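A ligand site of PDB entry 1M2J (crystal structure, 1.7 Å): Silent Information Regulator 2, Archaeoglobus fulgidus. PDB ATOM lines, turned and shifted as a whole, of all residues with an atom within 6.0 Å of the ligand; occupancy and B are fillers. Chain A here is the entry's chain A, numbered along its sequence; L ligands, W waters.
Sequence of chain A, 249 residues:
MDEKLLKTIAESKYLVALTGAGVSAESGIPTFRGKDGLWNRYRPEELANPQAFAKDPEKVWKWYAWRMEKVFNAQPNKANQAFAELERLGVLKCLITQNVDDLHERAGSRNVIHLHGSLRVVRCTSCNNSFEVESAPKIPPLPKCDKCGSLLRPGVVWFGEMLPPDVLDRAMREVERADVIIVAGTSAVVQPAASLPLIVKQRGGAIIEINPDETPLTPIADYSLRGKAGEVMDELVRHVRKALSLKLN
The side-chain amide oxygen of Asn 211 lies within hydrogen-bond range of an oxygen (O1) of the ligand, 2.8 Å away.
O5 of the ligand lies within hydrogen-bond range of N of Arg 33 (2.7 Å).
N of Ala 229 lies within hydrogen-bond range of N1 of the ligand (2.8 Å).
The side-chain hydroxyl (OG) of Ser 187 is in hydrogen-bond range of an oxygen (O6) of the ligand, at 2.6 Å.
O14 of the ligand is in hydrogen-bond range of ND1 of His 116.
The backbone NH of Ala 21 sits at hydrogen-bond distance from an oxygen (O9) of the ligand (2.8 Å).
An oxygen (O12) of the ligand sits at hydrogen-bond distance from the indole nitrogen of Trp 39, at 2.8 Å.
O6 of the ligand is in salt-bridge range of NH2 of Arg 33, 2.7 Å away.
O5 of the ligand sits at hydrogen-bond distance from N of Phe 32, 2.8 Å away.
N of Ser 187 sits at hydrogen-bond distance from O8 of the ligand, at 3.0 Å.
A nitrogen (N3) of the ligand is in hydrogen-bond range of the side-chain carboxylate (OE2) of Glu 26 (3.1 Å).
O of Gln 98 is in hydrogen-bond range of O14 of the ligand (3.1 Å).
OD2 of Asp 213 is in hydrogen-bond range of O1 of the ligand (3.1 Å).
OG1 of Thr 186 lies within hydrogen-bond range of O8 of the ligand (2.6 Å).
N of Asp 213 is in hydrogen-bond range of OD1 of Asn 211, at 2.8 Å.
N of Trp 39 sits at hydrogen-bond distance from O of Phe 32 (2.9 Å).
O of Thr 19 lies within hydrogen-bond range of N of Gln 98, 3.1 Å away.
The backbone NH (N) of Ala 229 is in hydrogen-bond range of the side-chain carboxylate (OE2) of Glu 26, at 3.4 Å.
The backbone NH (N) of Ala 21 is in hydrogen-bond range of the side-chain amide oxygen (OD1) of Asn 99.
The side-chain hydroxyl of Thr 186 sits at hydrogen-bond distance from the side-chain amide nitrogen of Gln 98.
O of Gly 20 is in hydrogen-bond range of ND2 of Asn 99 (3.0 Å).
The backbone NH (N) of Gly 22 is in hydrogen-bond range of the backbone carbonyl oxygen (O) of Gly 185 (2.8 Å).
O of Gly 22 sits close to N1 of the ligand, 3.4 Å away.
O3 of the ligand sits close to O of Gly 185 (3.4 Å).
Gly 20 touches the ligand.
CB of Ala 25 touches N4 of the ligand (3.95 Å).
Thr 31 touches the ligand (CB to O5, 3.4 Å).
CZ of Phe 159 touches O12 of the ligand, at 3.4 Å.
CG2 of Val 190 touches O11 of the ligand (3.4 Å).
CD of Pro 212 touches N2 of the ligand (3.3 Å).
Lys 228 touches the ligand.
Hydrophobic or aromatic side chains that line the ligand: Ala 21, Ala 25, Phe 32, Trp 39, His 116, Phe 159, Val 190, Pro 212 and Ala 229.
Of the 33 residues printed, 21 come within 4 Å of the ligand.
The nearest printed residue that does not touch the ligand is Asn 99 (4.2 Å).
Water W3 lies within hydrogen-bond range of an oxygen (O2) of the ligand (2.7 Å) and the side-chain carboxylate (OD2) of Asp 213 (3.1 Å).
Water W7 lies within hydrogen-bond range of O9 of the ligand (2.7 Å), OD1 of Asn 99 (2.7 Å), O of Gln 98 (3.3 Å) and N of Ala 21 (3.4 Å).
Water W5 bridges O of Gln 98 and O14 of the ligand.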
ATOM      1  N   THR A  19       5.797  16.712   7.167  1.00  0.00           N
ATOM      2  CA  THR A  19       6.128  15.299   7.089  1.00  0.00           C
ATOM      3  C   THR A  19       7.546  15.062   6.602  1.00  0.00           C
ATOM      4  O   THR A  19       8.140  15.902   5.914  1.00  0.00           O
ATOM      5  CB  THR A  19       5.175  14.522   6.139  1.00  0.00           C
ATOM      6  OG1 THR A  19       5.302  15.024   4.810  1.00  0.00           O
ATOM      7  CG2 THR A  19       3.727  14.642   6.608  1.00  0.00           C
ATOM      8  N   GLY A  20       8.070  13.901   6.982  1.00  0.00           N
ATOM      9  CA  GLY A  20       9.409  13.493   6.594  1.00  0.00           C
ATOM     10  C   GLY A  20       9.416  12.085   6.029  1.00  0.00           C
ATOM     11  O   GLY A  20       8.358  11.481   5.832  1.00  0.00           O
ATOM     12  N   ALA A  21      10.611  11.552   5.784  1.00  0.00           N
ATOM     13  CA  ALA A  21      10.775  10.228   5.199  1.00  0.00           C
ATOM     14  C   ALA A  21      10.049   9.087   5.913  1.00  0.00           C
ATOM     15  O   ALA A  21       9.719   8.075   5.284  1.00  0.00           O
ATOM     16  CB  ALA A  21      12.258   9.891   5.085  1.00  0.00           C
ATOM     17  N   GLY A  22       9.813   9.245   7.208  1.00  0.00           N
ATOM     18  CA  GLY A  22       9.125   8.211   7.959  1.00  0.00           C
ATOM     19  C   GLY A  22       7.706   7.961   7.493  1.00  0.00           C
ATOM     20  O   GLY A  22       7.161   6.874   7.676  1.00  0.00           O
ATOM     21  N   VAL A  23       7.076   8.970   6.887  1.00  0.00           N
ATOM     22  CA  VAL A  23       5.708   8.818   6.432  1.00  0.00           C
ATOM     23  C   VAL A  23       5.627   8.001   5.141  1.00  0.00           C
ATOM     24  O   VAL A  23       4.556   7.545   4.742  1.00  0.00           O
ATOM     25  CB  VAL A  23       5.035  10.190   6.237  1.00  0.00           C
ATOM     26  CG1 VAL A  23       3.595  10.020   5.766  1.00  0.00           C
ATOM     27  CG2 VAL A  23       5.054  10.960   7.556  1.00  0.00           C
ATOM     28  N   ALA A  25       7.912   5.429   4.704  1.00  0.00           N
ATOM     29  CA  ALA A  25       8.527   4.162   5.072  1.00  0.00           C
ATOM     30  C   ALA A  25       7.595   2.957   4.937  1.00  0.00           C
ATOM     31  O   ALA A  25       8.044   1.872   4.563  1.00  0.00           O
ATOM     32  CB  ALA A  25       9.061   4.234   6.498  1.00  0.00           C
ATOM     33  N   GLU A  26       6.322   3.141   5.248  1.00  0.00           N
ATOM     34  CA  GLU A  26       5.361   2.041   5.149  1.00  0.00           C
ATOM     35  C   GLU A  26       4.969   1.703   3.713  1.00  0.00           C
ATOM     36  O   GLU A  26       4.126   0.838   3.471  1.00  0.00           O
ATOM     37  CB  GLU A  26       4.149   2.344   6.020  1.00  0.00           C
ATOM     38  CG  GLU A  26       4.493   2.318   7.514  1.00  0.00           C
ATOM     39  CD  GLU A  26       3.425   2.909   8.405  1.00  0.00           C
ATOM     40  OE1 GLU A  26       2.337   2.306   8.535  1.00  0.00           O
ATOM     41  OE2 GLU A  26       3.671   3.983   9.002  1.00  0.00           O
ATOM     42  N   THR A  31      14.122   5.085   4.987  1.00  0.00           N
ATOM     43  CA  THR A  31      14.332   6.465   5.425  1.00  0.00           C
ATOM     44  C   THR A  31      15.794   6.815   5.183  1.00  0.00           C
ATOM     45  O   THR A  31      16.564   5.998   4.689  1.00  0.00           O
ATOM     46  CB  THR A  31      14.012   6.630   6.913  1.00  0.00           C
ATOM     47  OG1 THR A  31      14.819   5.734   7.690  1.00  0.00           O
ATOM     48  CG2 THR A  31      12.540   6.349   7.182  1.00  0.00           C
ATOM     49  N   PHE A  32      16.169   8.041   5.535  1.00  0.00           N
ATOM     50  CA  PHE A  32      17.542   8.481   5.339  1.00  0.00           C
ATOM     51  C   PHE A  32      18.415   8.126   6.525  1.00  0.00           C
ATOM     52  O   PHE A  32      19.566   7.718   6.372  1.00  0.00           O
ATOM     53  CB  PHE A  32      17.590   9.992   5.114  1.00  0.00           C
ATOM     54  CG  PHE A  32      16.960  10.424   3.825  1.00  0.00           C
ATOM     55  CD1 PHE A  32      17.634  10.262   2.624  1.00  0.00           C
ATOM     56  CD2 PHE A  32      15.677  10.954   3.803  1.00  0.00           C
ATOM     57  CE1 PHE A  32      17.041  10.620   1.411  1.00  0.00           C
ATOM     58  CE2 PHE A  32      15.072  11.317   2.608  1.00  0.00           C
ATOM     59  CZ  PHE A  32      15.752  11.143   1.404  1.00  0.00           C
ATOM     60  N   ARG A  33      17.862   8.277   7.722  1.00  0.00           N
ATOM     61  CA  ARG A  33      18.606   7.997   8.931  1.00  0.00           C
ATOM     62  C   ARG A  33      17.983   6.877   9.736  1.00  0.00           C
ATOM     63  O   ARG A  33      16.852   6.456   9.472  1.00  0.00           O
ATOM     64  CB  ARG A  33      18.731   9.281   9.743  1.00  0.00           C
ATOM     65  CG  ARG A  33      19.289  10.428   8.896  1.00  0.00           C
ATOM     66  CD  ARG A  33      19.416  11.755   9.634  1.00  0.00           C
ATOM     67  NE  ARG A  33      20.019  12.769   8.758  1.00  0.00           N
ATOM     68  CZ  ARG A  33      19.397  13.355   7.745  1.00  0.00           C
ATOM     69  NH1 ARG A  33      20.020  14.256   7.002  1.00  0.00           N
ATOM     70  NH2 ARG A  33      18.130  13.059   7.482  1.00  0.00           N
ATOM     71  N   GLY A  34      18.729   6.371  10.714  1.00  0.00           N
ATOM     72  CA  GLY A  34      18.227   5.284  11.537  1.00  0.00           C
ATOM     73  C   GLY A  34      18.840   3.971  11.112  1.00  0.00           C
ATOM     74  O   GLY A  34      19.850   3.930  10.407  1.00  0.00           O
ATOM     75  N   TRP A  39      21.362   7.078   4.198  1.00  0.00           N
ATOM     76  CA  TRP A  39      22.593   7.786   4.499  1.00  0.00           C
ATOM     77  C   TRP A  39      23.538   6.949   5.352  1.00  0.00           C
ATOM     78  O   TRP A  39      24.694   7.312   5.574  1.00  0.00           O
ATOM     79  CB  TRP A  39      22.293   9.115   5.206  1.00  0.00           C
ATOM     80  CG  TRP A  39      21.634  10.159   4.333  1.00  0.00           C
ATOM     81  CD1 TRP A  39      21.003  11.299   4.766  1.00  0.00           C
ATOM     82  CD2 TRP A  39      21.585  10.201   2.892  1.00  0.00           C
ATOM     83  NE1 TRP A  39      20.565  12.036   3.687  1.00  0.00           N
ATOM     84  CE2 TRP A  39      20.900  11.388   2.534  1.00  0.00           C
ATOM     85  CE3 TRP A  39      22.040   9.344   1.880  1.00  0.00           C
ATOM     86  CZ2 TRP A  39      20.672  11.744   1.196  1.00  0.00           C
ATOM     87  CZ3 TRP A  39      21.809   9.704   0.551  1.00  0.00           C
ATOM     88  CH2 TRP A  39      21.130  10.887   0.221  1.00  0.00           C
ATOM     89  N   GLN A  98       9.126  17.296   3.385  1.00  0.00           N
ATOM     90  CA  GLN A  98      10.548  17.324   3.081  1.00  0.00           C
ATOM     91  C   GLN A  98      10.815  16.186   2.095  1.00  0.00           C
ATOM     92  O   GLN A  98      11.922  16.050   1.576  1.00  0.00           O
ATOM     93  CB  GLN A  98      11.374  17.096   4.347  1.00  0.00           C
ATOM     94  CG  GLN A  98      11.174  18.136   5.443  1.00  0.00           C
ATOM     95  CD  GLN A  98      11.811  17.695   6.751  1.00  0.00           C
ATOM     96  OE1 GLN A  98      13.025  17.792   6.922  1.00  0.00           O
ATOM     97  NE2 GLN A  98      10.988  17.180   7.657  1.00  0.00           N
ATOM     98  N   ASN A  99       9.798  15.369   1.859  1.00  0.00           N
ATOM     99  CA  ASN A  99       9.931  14.222   0.957  1.00  0.00           C
ATOM    100  C   ASN A  99       9.996  14.597  -0.510  1.00  0.00           C
ATOM    101  O   ASN A  99       9.306  15.519  -0.957  1.00  0.00           O
ATOM    102  CB  ASN A  99       8.780  13.230   1.181  1.00  0.00           C
ATOM    103  CG  ASN A  99       8.706  12.732   2.601  1.00  0.00           C
ATOM    104  OD1 ASN A  99       9.731  12.688   3.307  1.00  0.00           O
ATOM    105  ND2 ASN A  99       7.520  12.342   3.045  1.00  0.00           N
ATOM    106  N   HIS A 116      11.982  20.333  -0.248  1.00  0.00           N
ATOM    107  CA  HIS A 116      13.233  19.854  -0.824  1.00  0.00           C
ATOM    108  C   HIS A 116      13.162  19.365  -2.267  1.00  0.00           C
ATOM    109  O   HIS A 116      14.003  18.596  -2.716  1.00  0.00           O
ATOM    110  CB  HIS A 116      13.805  18.744   0.071  1.00  0.00           C
ATOM    111  CG  HIS A 116      14.037  19.160   1.484  1.00  0.00           C
ATOM    112  ND1 HIS A 116      14.269  18.261   2.500  1.00  0.00           N
ATOM    113  CD2 HIS A 116      14.093  20.394   2.063  1.00  0.00           C
ATOM    114  CE1 HIS A 116      14.469  18.909   3.634  1.00  0.00           C
ATOM    115  NE2 HIS A 116      14.369  20.203   3.393  1.00  0.00           N
ATOM    116  N   VAL A 157      16.592  19.305  -3.751  1.00  0.00           N
ATOM    117  CA  VAL A 157      17.539  20.180  -3.077  1.00  0.00           C
ATOM    118  C   VAL A 157      18.617  19.359  -2.372  1.00  0.00           C
ATOM    119  O   VAL A 157      18.309  18.480  -1.565  1.00  0.00           O
ATOM    120  CB  VAL A 157      16.829  21.076  -2.023  1.00  0.00           C
ATOM    121  CG1 VAL A 157      17.846  21.973  -1.323  1.00  0.00           C
ATOM    122  CG2 VAL A 157      15.763  21.922  -2.705  1.00  0.00           C
ATOM    123  N   PHE A 159      22.433  19.084  -0.119  1.00  0.00           N
ATOM    124  CA  PHE A 159      23.067  19.752   1.010  1.00  0.00           C
ATOM    125  C   PHE A 159      23.881  20.956   0.550  1.00  0.00           C
ATOM    126  O   PHE A 159      24.597  20.887  -0.449  1.00  0.00           O
ATOM    127  CB  PHE A 159      23.978  18.789   1.779  1.00  0.00           C
ATOM    128  CG  PHE A 159      23.240  17.752   2.569  1.00  0.00           C
ATOM    129  CD1 PHE A 159      22.877  16.538   1.997  1.00  0.00           C
ATOM    130  CD2 PHE A 159      22.888  18.004   3.901  1.00  0.00           C
ATOM    131  CE1 PHE A 159      22.165  15.587   2.729  1.00  0.00           C
ATOM    132  CE2 PHE A 159      22.170  17.065   4.636  1.00  0.00           C
ATOM    133  CZ  PHE A 159      21.809  15.847   4.056  1.00  0.00           C
ATOM    134  N   ALA A 184       5.129  14.584  11.498  1.00  0.00           N
ATOM    135  CA  ALA A 184       5.242  13.143  11.381  1.00  0.00           C
ATOM    136  C   ALA A 184       6.385  12.613  10.527  1.00  0.00           C
ATOM    137  O   ALA A 184       6.688  13.146   9.466  1.00  0.00           O
ATOM    138  CB  ALA A 184       3.932  12.591  10.849  1.00  0.00           C
ATOM    139  N   GLY A 185       6.998  11.544  11.011  1.00  0.00           N
ATOM    140  CA  GLY A 185       8.068  10.900  10.272  1.00  0.00           C
ATOM    141  C   GLY A 185       9.308  11.704   9.944  1.00  0.00           C
ATOM    142  O   GLY A 185       9.895  11.520   8.881  1.00  0.00           O
ATOM    143  N   THR A 186       9.721  12.602  10.839  1.00  0.00           N
ATOM    144  CA  THR A 186      10.929  13.374  10.571  1.00  0.00           C
ATOM    145  C   THR A 186      11.800  13.394  11.813  1.00  0.00           C
ATOM    146  O   THR A 186      11.308  13.480  12.944  1.00  0.00           O
ATOM    147  CB  THR A 186      10.604  14.818  10.083  1.00  0.00           C
ATOM    148  OG1 THR A 186      11.827  15.525   9.847  1.00  0.00           O
ATOM    149  CG2 THR A 186       9.746  15.575  11.096  1.00  0.00           C
ATOM    150  N   SER A 187      13.110  13.288  11.592  1.00  0.00           N
ATOM    151  CA  SER A 187      14.092  13.259  12.673  1.00  0.00           C
ATOM    152  C   SER A 187      14.396  14.615  13.300  1.00  0.00           C
ATOM    153  O   SER A 187      15.151  14.704  14.261  1.00  0.00           O
ATOM    154  CB  SER A 187      15.391  12.606  12.178  1.00  0.00           C
ATOM    155  OG  SER A 187      15.901  13.314  11.064  1.00  0.00           O
ATOM    156  N   ALA A 188      13.816  15.666  12.725  1.00  0.00           N
ATOM    157  CA  ALA A 188      13.985  17.032  13.234  1.00  0.00           C
ATOM    158  C   ALA A 188      15.428  17.516  13.431  1.00  0.00           C
ATOM    159  O   ALA A 188      15.753  18.118  14.452  1.00  0.00           O
ATOM    160  CB  ALA A 188      13.228  17.187  14.553  1.00  0.00           C
ATOM    161  N   VAL A 189      16.289  17.247  12.453  1.00  0.00           N
ATOM    162  CA  VAL A 189      17.675  17.687  12.546  1.00  0.00           C
ATOM    163  C   VAL A 189      18.079  18.554  11.360  1.00  0.00           C
ATOM    164  O   VAL A 189      18.866  19.480  11.506  1.00  0.00           O
ATOM    165  CB  VAL A 189      18.649  16.484  12.676  1.00  0.00           C
ATOM    166  CG1 VAL A 189      18.425  15.779  14.002  1.00  0.00           C
ATOM    167  CG2 VAL A 189      18.462  15.532  11.517  1.00  0.00           C
ATOM    168  N   VAL A 190      17.512  18.263  10.193  1.00  0.00           N
ATOM    169  CA  VAL A 190      17.833  19.027   8.995  1.00  0.00           C
ATOM    170  C   VAL A 190      17.122  20.384   8.980  1.00  0.00           C
ATOM    171  O   VAL A 190      15.911  20.463   9.154  1.00  0.00           O
ATOM    172  CB  VAL A 190      17.445  18.253   7.720  1.00  0.00           C
ATOM    173  CG1 VAL A 190      17.636  19.127   6.498  1.00  0.00           C
ATOM    174  CG2 VAL A 190      18.284  16.993   7.607  1.00  0.00           C
ATOM    175  N   ILE A 210       4.473  12.696  15.674  1.00  0.00           N
ATOM    176  CA  ILE A 210       4.199  11.289  15.442  1.00  0.00           C
ATOM    177  C   ILE A 210       5.493  10.662  14.930  1.00  0.00           C
ATOM    178  O   ILE A 210       5.919  10.932  13.805  1.00  0.00           O
ATOM    179  CB  ILE A 210       3.092  11.093  14.390  1.00  0.00           C
ATOM    180  CG1 ILE A 210       1.795  11.760  14.865  1.00  0.00           C
ATOM    181  CG2 ILE A 210       2.870   9.612  14.166  1.00  0.00           C
ATOM    182  CD1 ILE A 210       0.690  11.731  13.829  1.00  0.00           C
ATOM    183  N   ASN A 211       6.102   9.825  15.748  1.00  0.00           N
ATOM    184  CA  ASN A 211       7.369   9.215  15.375  1.00  0.00           C
ATOM    185  C   ASN A 211       7.679   8.075  16.340  1.00  0.00           C
ATOM    186  O   ASN A 211       7.505   8.227  17.556  1.00  0.00           O
ATOM    187  CB  ASN A 211       8.458  10.285  15.459  1.00  0.00           C
ATOM    188  CG  ASN A 211       9.750   9.878  14.775  1.00  0.00           C
ATOM    189  OD1 ASN A 211      10.247   8.768  14.964  1.00  0.00           O
ATOM    190  ND2 ASN A 211      10.321  10.803  13.995  1.00  0.00           N
ATOM    191  N   PRO A 212       8.128   6.918  15.832  1.00  0.00           N
ATOM    192  CA  PRO A 212       8.452   5.798  16.717  1.00  0.00           C
ATOM    193  C   PRO A 212       9.645   6.122  17.625  1.00  0.00           C
ATOM    194  O   PRO A 212       9.828   5.486  18.661  1.00  0.00           O
ATOM    195  CB  PRO A 212       8.744   4.659  15.748  1.00  0.00           C
ATOM    196  CG  PRO A 212       9.234   5.360  14.528  1.00  0.00           C
ATOM    197  CD  PRO A 212       8.291   6.532  14.423  1.00  0.00           C
ATOM    198  N   ASP A 213      10.435   7.110  17.233  1.00  0.00           N
ATOM    199  CA  ASP A 213      11.588   7.543  18.020  1.00  0.00           C
ATOM    200  C   ASP A 213      11.349   8.934  18.571  1.00  0.00           C
ATOM    201  O   ASP A 213      10.498   9.680  18.079  1.00  0.00           O
ATOM    202  CB  ASP A 213      12.860   7.599  17.167  1.00  0.00           C
ATOM    203  CG  ASP A 213      13.284   6.250  16.629  1.00  0.00           C
ATOM    204  OD1 ASP A 213      12.977   5.223  17.254  1.00  0.00           O
ATOM    205  OD2 ASP A 213      13.958   6.224  15.571  1.00  0.00           O
ATOM    206  N   THR A 215      12.810  12.723  19.213  1.00  0.00           N
ATOM    207  CA  THR A 215      13.689  13.586  18.427  1.00  0.00           C
ATOM    208  C   THR A 215      13.983  14.886  19.193  1.00  0.00           C
ATOM    209  O   THR A 215      13.483  15.087  20.300  1.00  0.00           O
ATOM    210  CB  THR A 215      13.041  13.996  17.088  1.00  0.00           C
ATOM    211  OG1 THR A 215      12.061  15.017  17.318  1.00  0.00           O
ATOM    212  CG2 THR A 215      12.358  12.806  16.423  1.00  0.00           C
ATOM    213  N   GLY A 227       4.694   5.801  17.691  1.00  0.00           N
ATOM    214  CA  GLY A 227       4.116   4.775  16.840  1.00  0.00           C
ATOM    215  C   GLY A 227       4.305   5.132  15.375  1.00  0.00           C
ATOM    216  O   GLY A 227       4.785   6.223  15.046  1.00  0.00           O
ATOM    217  N   LYS A 228       3.933   4.208  14.506  1.00  0.00           N
ATOM    218  CA  LYS A 228       4.065   4.422  13.068  1.00  0.00           C
ATOM    219  C   LYS A 228       2.972   5.362  12.573  1.00  0.00           C
ATOM    220  O   LYS A 228       1.851   5.349  13.073  1.00  0.00           O
ATOM    221  CB  LYS A 228       4.003   3.098  12.317  1.00  0.00           C
ATOM    222  CG  LYS A 228       5.189   2.194  12.595  1.00  0.00           C
ATOM    223  CD  LYS A 228       5.161   0.964  11.698  1.00  0.00           C
ATOM    224  CE  LYS A 228       6.423   0.126  11.868  1.00  0.00           C
ATOM    225  NZ  LYS A 228       6.416  -1.074  10.993  1.00  0.00           N
ATOM    226  N   ALA A 229       3.305   6.171  11.576  1.00  0.00           N
ATOM    227  CA  ALA A 229       2.375   7.131  11.007  1.00  0.00           C
ATOM    228  C   ALA A 229       1.107   6.480  10.474  1.00  0.00           C
ATOM    229  O   ALA A 229       0.012   7.035  10.608  1.00  0.00           O
ATOM    230  CB  ALA A 229       3.048   7.921   9.902  1.00  0.00           C
ATOM    231  N   GLY A 230       1.256   5.322   9.844  1.00  0.00           N
ATOM    232  CA  GLY A 230       0.105   4.640   9.283  1.00  0.00           C
ATOM    233  C   GLY A 230      -0.965   4.338  10.328  1.00  0.00           C
ATOM    234  O   GLY A 230      -2.109   4.773  10.191  1.00  0.00           O
HETATM  235  N1  LIG L   1       6.060   6.284  10.857  1.00  0.00           N
HETATM  236  C1  LIG L   1       6.482   7.531  11.312  1.00  0.00           C
HETATM  237  N2  LIG L   1       7.849   7.800  11.434  1.00  0.00           N
HETATM  238  C2  LIG L   1       8.773   6.818  11.097  1.00  0.00           C
HETATM  239  C3  LIG L   1       8.360   5.575  10.640  1.00  0.00           C
HETATM  240  C4  LIG L   1       6.974   5.275  10.510  1.00  0.00           C
HETATM  241  N3  LIG L   1       6.528   4.076  10.067  1.00  0.00           N
HETATM  242  N4  LIG L   1       9.437   4.837  10.388  1.00  0.00           N
HETATM  243  C5  LIG L   1      10.510   5.626  10.689  1.00  0.00           C
HETATM  244  N5  LIG L   1      10.166   6.938  11.148  1.00  0.00           N
HETATM  245  C6  LIG L   1      10.881   8.096  11.554  1.00  0.00           C
HETATM  246  C7  LIG L   1      12.167   7.812  12.128  1.00  0.00           C
HETATM  247  O1  LIG L   1      12.170   7.416  13.395  1.00  0.00           O
HETATM  248  C8  LIG L   1      12.891   9.013  11.853  1.00  0.00           C
HETATM  249  O2  LIG L   1      12.901   9.865  12.894  1.00  0.00           O
HETATM  250  O3  LIG L   1      11.166   8.828  10.474  1.00  0.00           O
HETATM  251  C9  LIG L   1      12.211   9.646  10.764  1.00  0.00           C
HETATM  252  C10 LIG L   1      12.982   9.848   9.538  1.00  0.00           C
HETATM  253  O4  LIG L   1      14.038  10.650   9.757  1.00  0.00           O
HETATM  254  P1  LIG L   1      14.957  10.959   8.438  1.00  0.00           P
HETATM  255  O5  LIG L   1      15.468   9.607   7.765  1.00  0.00           O
HETATM  256  O6  LIG L   1      16.175  11.870   8.873  1.00  0.00           O
HETATM  257  O7  LIG L   1      14.030  11.683   7.324  1.00  0.00           O
HETATM  258  P2  LIG L   1      13.776  13.292   7.298  1.00  0.00           P
HETATM  259  O8  LIG L   1      13.579  13.934   8.722  1.00  0.00           O
HETATM  260  O9  LIG L   1      12.511  13.524   6.391  1.00  0.00           O
HETATM  261  O10 LIG L   1      15.098  13.892   6.552  1.00  0.00           O
HETATM  262  C11 LIG L   1      15.160  15.193   6.352  1.00  0.00           C
HETATM  263  O11 LIG L   1      17.190  14.899   5.194  1.00  0.00           O
HETATM  264  O12 LIG L   1      18.837  14.269   3.816  1.00  0.00           O
HETATM  265  C12 LIG L   1      17.461  14.131   4.196  1.00  0.00           C
HETATM  266  O13 LIG L   1      16.807  15.836   2.348  1.00  0.00           O
HETATM  267  C13 LIG L   1      16.649  14.772   3.098  1.00  0.00           C
HETATM  268  O14 LIG L   1      14.392  15.392   3.366  1.00  0.00           O
HETATM  269  C14 LIG L   1      15.470  14.838   3.942  1.00  0.00           C
HETATM  270  C15 LIG L   1      15.966  15.417   5.145  1.00  0.00           C
HETATM  271  O   HOH W   1      10.587   2.499   9.464  1.00  0.00           O
HETATM  272  O   HOH W   2       8.032   1.850   9.255  1.00  0.00           O
HETATM  273  O   HOH W   3      14.679   9.098  14.712  1.00  0.00           O
HETATM  274  O   HOH W   4      15.576  15.919   9.997  1.00  0.00           O
HETATM  275  O   HOH W   5      13.544  13.867   0.703  1.00  0.00           O
HETATM  276  O   HOH W   6      15.487   7.005  11.685  1.00  0.00           O
HETATM  277  O   HOH W   7      12.287  13.613   3.717  1.00  0.00           O
